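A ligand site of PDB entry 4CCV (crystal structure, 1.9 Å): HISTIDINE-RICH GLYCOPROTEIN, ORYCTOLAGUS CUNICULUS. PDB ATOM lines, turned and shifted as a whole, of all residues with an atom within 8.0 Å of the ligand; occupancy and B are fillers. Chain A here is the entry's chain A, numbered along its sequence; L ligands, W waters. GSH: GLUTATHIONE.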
ATOM      1  N   ARG A  15     -27.664  22.095  23.295  1.00  0.00           N
ATOM      2  CA  ARG A  15     -27.391  22.484  21.923  1.00  0.00           C
ATOM      3  C   ARG A  15     -28.267  23.605  21.448  1.00  0.00           C
ATOM      4  O   ARG A  15     -27.800  24.552  20.842  1.00  0.00           O
ATOM      5  CB  ARG A  15     -27.489  21.303  20.920  1.00  0.00           C
ATOM      6  CG  ARG A  15     -26.835  21.758  19.623  1.00  0.00           C
ATOM      7  CD  ARG A  15     -26.709  20.659  18.562  1.00  0.00           C
ATOM      8  NE  ARG A  15     -26.045  21.275  17.418  1.00  0.00           N
ATOM      9  CZ  ARG A  15     -24.750  21.164  17.124  1.00  0.00           C
ATOM     10  NH1 ARG A  15     -23.947  20.392  17.857  1.00  0.00           N
ATOM     11  NH2 ARG A  15     -24.285  21.802  16.065  1.00  0.00           N
ATOM     12  N   SER A  34     -22.782  34.756   9.277  1.00  0.00           N
ATOM     13  CA  SER A  34     -22.799  33.431   8.652  1.00  0.00           C
ATOM     14  C   SER A  34     -22.490  32.288   9.632  1.00  0.00           C
ATOM     15  O   SER A  34     -22.358  31.139   9.215  1.00  0.00           O
ATOM     16  CB  SER A  34     -21.740  33.377   7.532  1.00  0.00           C
ATOM     17  OG  SER A  34     -20.446  33.310   8.133  1.00  0.00           O
ATOM     18  N   PHE A  35     -22.336  32.566  10.924  1.00  0.00           N
ATOM     19  CA  PHE A  35     -21.757  31.580  11.823  1.00  0.00           C
ATOM     20  C   PHE A  35     -22.790  30.500  12.258  1.00  0.00           C
ATOM     21  O   PHE A  35     -23.992  30.781  12.347  1.00  0.00           O
ATOM     22  CB  PHE A  35     -21.112  32.260  13.051  1.00  0.00           C
ATOM     23  CG  PHE A  35     -19.698  32.727  12.852  1.00  0.00           C
ATOM     24  CD1 PHE A  35     -19.365  33.679  11.904  1.00  0.00           C
ATOM     25  CD2 PHE A  35     -18.690  32.245  13.666  1.00  0.00           C
ATOM     26  CE1 PHE A  35     -18.045  34.115  11.738  1.00  0.00           C
ATOM     27  CE2 PHE A  35     -17.384  32.697  13.551  1.00  0.00           C
ATOM     28  CZ  PHE A  35     -17.049  33.619  12.576  1.00  0.00           C
ATOM     29  N   ARG A  36     -22.311  29.280  12.498  1.00  0.00           N
ATOM     30  CA  ARG A  36     -23.146  28.184  13.026  1.00  0.00           C
ATOM     31  C   ARG A  36     -22.396  27.403  14.086  1.00  0.00           C
ATOM     32  O   ARG A  36     -21.185  27.414  14.100  1.00  0.00           O
ATOM     33  CB  ARG A  36     -23.535  27.251  11.905  1.00  0.00           C
ATOM     34  CG  ARG A  36     -24.277  27.971  10.819  1.00  0.00           C
ATOM     35  CD  ARG A  36     -24.690  26.926   9.808  1.00  0.00           C
ATOM     36  NE  ARG A  36     -25.499  27.459   8.712  1.00  0.00           N
ATOM     37  CZ  ARG A  36     -25.910  26.726   7.682  1.00  0.00           C
ATOM     38  NH1 ARG A  36     -25.584  25.427   7.594  1.00  0.00           N
ATOM     39  NH2 ARG A  36     -26.653  27.281   6.734  1.00  0.00           N
ATOM     40  N   VAL A  37     -23.125  26.808  15.028  1.00  0.00           N
ATOM     41  CA  VAL A  37     -22.534  26.049  16.119  1.00  0.00           C
ATOM     42  C   VAL A  37     -21.978  24.789  15.518  1.00  0.00           C
ATOM     43  O   VAL A  37     -22.665  24.139  14.685  1.00  0.00           O
ATOM     44  CB  VAL A  37     -23.656  25.675  17.171  1.00  0.00           C
ATOM     45  CG1 VAL A  37     -23.104  24.664  18.181  1.00  0.00           C
ATOM     46  CG2 VAL A  37     -24.075  26.974  17.819  1.00  0.00           C
ATOM     47  N   ASP A  38     -20.752  24.454  15.943  1.00  0.00           N
ATOM     48  CA  ASP A  38     -20.100  23.216  15.530  1.00  0.00           C
ATOM     49  C   ASP A  38     -20.510  22.168  16.607  1.00  0.00           C
ATOM     50  O   ASP A  38     -21.426  21.373  16.342  1.00  0.00           O
ATOM     51  CB  ASP A  38     -18.590  23.410  15.379  1.00  0.00           C
ATOM     52  CG  ASP A  38     -17.919  22.226  14.668  1.00  0.00           C
ATOM     53  OD1 ASP A  38     -18.577  21.163  14.541  1.00  0.00           O
ATOM     54  OD2 ASP A  38     -16.739  22.377  14.243  1.00  0.00           O
ATOM     55  N   ARG A  39     -19.863  22.153  17.783  1.00  0.00           N
ATOM     56  CA  ARG A  39     -20.143  21.157  18.835  1.00  0.00           C
ATOM     57  C   ARG A  39     -20.285  21.909  20.153  1.00  0.00           C
ATOM     58  O   ARG A  39     -19.557  22.897  20.378  1.00  0.00           O
ATOM     59  CB  ARG A  39     -18.982  20.187  19.069  1.00  0.00           C
ATOM     60  CG  ARG A  39     -18.676  19.259  17.921  1.00  0.00           C
ATOM     61  CD  ARG A  39     -17.545  18.288  18.187  1.00  0.00           C
ATOM     62  NE  ARG A  39     -17.230  17.645  16.892  1.00  0.00           N
ATOM     63  CZ  ARG A  39     -16.112  17.827  16.159  1.00  0.00           C
ATOM     64  NH1 ARG A  39     -15.094  18.557  16.622  1.00  0.00           N
ATOM     65  NH2 ARG A  39     -15.941  17.222  14.985  1.00  0.00           N
ATOM     66  N   SER A  59     -18.106  25.325  20.123  1.00  0.00           N
ATOM     67  CA  SER A  59     -17.328  25.704  18.973  1.00  0.00           C
ATOM     68  C   SER A  59     -18.275  26.223  17.922  1.00  0.00           C
ATOM     69  O   SER A  59     -19.453  25.839  17.912  1.00  0.00           O
ATOM     70  CB  SER A  59     -16.496  24.539  18.408  1.00  0.00           C
ATOM     71  OG  SER A  59     -17.234  23.364  18.409  1.00  0.00           O
ATOM     72  N   VAL A  60     -17.760  27.110  17.079  1.00  0.00           N
ATOM     73  CA  VAL A  60     -18.470  27.685  15.955  1.00  0.00           C
ATOM     74  C   VAL A  60     -17.651  27.638  14.662  1.00  0.00           C
ATOM     75  O   VAL A  60     -16.442  27.541  14.719  1.00  0.00           O
ATOM     76  CB  VAL A  60     -18.924  29.137  16.262  1.00  0.00           C
ATOM     77  CG1 VAL A  60     -19.923  29.120  17.429  1.00  0.00           C
ATOM     78  CG2 VAL A  60     -17.739  30.097  16.551  1.00  0.00           C
ATOM     79  N   ARG A  61     -18.325  27.744  13.505  1.00  0.00           N
ATOM     80  CA  ARG A  61     -17.684  27.863  12.215  1.00  0.00           C
ATOM     81  C   ARG A  61     -18.204  29.088  11.474  1.00  0.00           C
ATOM     82  O   ARG A  61     -19.381  29.423  11.550  1.00  0.00           O
ATOM     83  CB  ARG A  61     -17.975  26.643  11.329  1.00  0.00           C
ATOM     84  CG  ARG A  61     -17.352  25.358  11.813  1.00  0.00           C
ATOM     85  CD  ARG A  61     -15.844  25.468  11.952  1.00  0.00           C
ATOM     86  NE  ARG A  61     -15.229  24.147  12.153  1.00  0.00           N
ATOM     87  CZ  ARG A  61     -14.044  23.752  11.653  1.00  0.00           C
ATOM     88  NH1 ARG A  61     -13.326  24.593  10.903  1.00  0.00           N
ATOM     89  NH2 ARG A  61     -13.595  22.523  11.889  1.00  0.00           N
ATOM     90  N   ASN A  62     -17.304  29.723  10.745  1.00  0.00           N
ATOM     91  CA  ASN A  62     -17.628  30.866   9.901  1.00  0.00           C
ATOM     92  C   ASN A  62     -18.024  30.348   8.551  1.00  0.00           C
ATOM     93  O   ASN A  62     -17.138  30.076   7.691  1.00  0.00           O
ATOM     94  CB  ASN A  62     -16.385  31.764   9.774  1.00  0.00           C
ATOM     95  CG  ASN A  62     -16.668  33.012   8.991  1.00  0.00           C
ATOM     96  OD1 ASN A  62     -17.611  33.072   8.209  1.00  0.00           O
ATOM     97  ND2 ASN A  62     -15.846  34.030   9.182  1.00  0.00           N
ATOM     98  N   CYS A  63     -19.327  30.163   8.322  1.00  0.00           N
ATOM     99  CA  CYS A  63     -19.735  29.457   7.097  1.00  0.00           C
ATOM    100  C   CYS A  63     -19.477  30.238   5.825  1.00  0.00           C
ATOM    101  O   CYS A  63     -19.491  29.647   4.721  1.00  0.00           O
ATOM    102  CB  CYS A  63     -21.199  29.020   7.151  1.00  0.00           C
ATOM    103  SG  CYS A  63     -21.457  27.895   8.557  1.00  0.00           S
ATOM    104  N   SER A  64     -19.226  31.546   5.906  1.00  0.00           N
ATOM    105  CA  SER A  64     -18.907  32.247   4.660  1.00  0.00           C
ATOM    106  C   SER A  64     -17.521  31.766   4.149  1.00  0.00           C
ATOM    107  O   SER A  64     -17.251  31.775   2.914  1.00  0.00           O
ATOM    108  CB  SER A  64     -19.004  33.746   4.797  1.00  0.00           C
ATOM    109  OG  SER A  64     -17.880  34.275   5.417  1.00  0.00           O
ATOM    110  N   ARG A  65     -16.671  31.323   5.078  1.00  0.00           N
ATOM    111  CA  ARG A  65     -15.392  30.713   4.687  1.00  0.00           C
ATOM    112  C   ARG A  65     -15.500  29.286   4.148  1.00  0.00           C
ATOM    113  O   ARG A  65     -14.509  28.729   3.750  1.00  0.00           O
ATOM    114  CB  ARG A  65     -14.379  30.797   5.802  1.00  0.00           C
ATOM    115  CG  ARG A  65     -13.793  32.203   5.854  1.00  0.00           C
ATOM    116  CD  ARG A  65     -13.234  32.480   7.193  1.00  0.00           C
ATOM    117  NE  ARG A  65     -12.547  33.765   7.284  1.00  0.00           N
ATOM    118  CZ  ARG A  65     -11.233  33.917   7.378  1.00  0.00           C
ATOM    119  NH1 ARG A  65     -10.414  32.881   7.326  1.00  0.00           N
ATOM    120  NH2 ARG A  65     -10.736  35.139   7.521  1.00  0.00           N
ATOM    121  N   SER A  66     -16.704  28.690   4.068  1.00  0.00           N
ATOM    122  CA  SER A  66     -16.861  27.440   3.347  1.00  0.00           C
ATOM    123  C   SER A  66     -17.014  27.671   1.868  1.00  0.00           C
ATOM    124  O   SER A  66     -17.022  26.713   1.091  1.00  0.00           O
ATOM    125  CB  SER A  66     -18.046  26.615   3.841  1.00  0.00           C
ATOM    126  OG  SER A  66     -19.294  27.288   3.662  1.00  0.00           O
ATOM    127  N   HIS A  67     -17.146  28.931   1.445  1.00  0.00           N
ATOM    128  CA  HIS A  67     -17.286  29.218   0.032  1.00  0.00           C
ATOM    129  C   HIS A  67     -16.009  29.754  -0.512  1.00  0.00           C
ATOM    130  O   HIS A  67     -15.213  30.296   0.237  1.00  0.00           O
ATOM    131  CB  HIS A  67     -18.388  30.230  -0.189  1.00  0.00           C
ATOM    132  CG  HIS A  67     -19.670  29.822   0.433  1.00  0.00           C
ATOM    133  ND1 HIS A  67     -20.504  28.873  -0.123  1.00  0.00           N
ATOM    134  CD2 HIS A  67     -20.247  30.183   1.603  1.00  0.00           C
ATOM    135  CE1 HIS A  67     -21.543  28.688   0.659  1.00  0.00           C
ATOM    136  NE2 HIS A  67     -21.417  29.475   1.710  1.00  0.00           N
ATOM    137  N   ALA A  73     -11.853  28.934   9.258  1.00  0.00           N
ATOM    138  CA  ALA A  73     -11.935  29.648  10.522  1.00  0.00           C
ATOM    139  C   ALA A  73     -12.719  28.824  11.527  1.00  0.00           C
ATOM    140  O   ALA A  73     -13.358  27.791  11.168  1.00  0.00           O
ATOM    141  CB  ALA A  73     -12.436  31.084  10.358  1.00  0.00           C
HETATM  142  N1  GSH L   1     -18.790  21.900  10.430  1.00  0.00           N
HETATM  143  CA1 GSH L   1     -20.136  21.416  10.630  1.00  0.00           C
HETATM  144  C1  GSH L   1     -20.475  20.521   9.437  1.00  0.00           C
HETATM  145  O11 GSH L   1     -19.710  19.553   9.203  1.00  0.00           O
HETATM  146  O12 GSH L   1     -21.459  20.721   8.694  1.00  0.00           O
HETATM  147  CB1 GSH L   1     -20.918  22.677  10.956  1.00  0.00           C
HETATM  148  CG1 GSH L   1     -22.329  22.675  10.401  1.00  0.00           C
HETATM  149  CD1 GSH L   1     -22.464  23.416   9.082  1.00  0.00           C
HETATM  150  OE1 GSH L   1     -23.582  23.698   8.791  1.00  0.00           O
HETATM  151  N2  GSH L   1     -21.454  23.797   8.249  1.00  0.00           N
HETATM  152  CA2 GSH L   1     -21.790  24.550   7.038  1.00  0.00           C
HETATM  153  C2  GSH L   1     -22.403  23.757   5.898  1.00  0.00           C
HETATM  154  O2  GSH L   1     -22.995  24.391   5.022  1.00  0.00           O
HETATM  155  CB2 GSH L   1     -20.577  25.310   6.558  1.00  0.00           C
HETATM  156  SG2 GSH L   1     -19.932  26.242   7.993  1.00  0.00           S
HETATM  157  N3  GSH L   1     -22.220  22.415   5.864  1.00  0.00           N
HETATM  158  CA3 GSH L   1     -22.545  21.529   4.727  1.00  0.00           C
HETATM  159  C3  GSH L   1     -23.918  21.737   4.148  1.00  0.00           C
HETATM  160  O31 GSH L   1     -24.914  21.594   4.908  1.00  0.00           O
HETATM  161  O32 GSH L   1     -24.027  22.058   2.929  1.00  0.00           O
HETATM  162  O   HOH W   1     -25.457  23.624  10.686  1.00  0.00           O
HETATM  163  O   HOH W   2     -18.734  22.767   7.807  1.00  0.00           O
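A sulfur (SG2) of the ligand is bonded to the side-chain sulfur of Cys 63, at 2.3 Å.
The guanidinium group (NH1) of Arg 36 lies within hydrogen-bond range of an oxygen (OE1) of the ligand (2.9 Å).
The backbone carbonyl oxygen (O) of Cys 63 lies within hydrogen-bond range of the side-chain hydroxyl (OG) of Ser 66, 2.6 Å away.
The backbone carbonyl oxygen (O) of Ser 34 sits close to the backbone NH (N) of Cys 63 (3.3 Å).
O of Arg 36 is in hydrogen-bond range of N of Arg 61 (2.9 Å).
NE of Arg 61 lies within salt-bridge range of OD2 of Asp 38, at 3.1 Å.
The guanidinium group of Arg 61 lies within hydrogen-bond range of the backbone carbonyl oxygen of Ala 73 (3.2 Å).
Arg 61 touches the ligand.
Ser 66 touches the ligand (OG to CB2, 3.7 Å).
Within 4 Å of the ligand: Arg 36, Arg 61, Cys 63 and Ser 66.
The nearest printed residue that does not touch the ligand is Asp 38 (4.2 Å).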
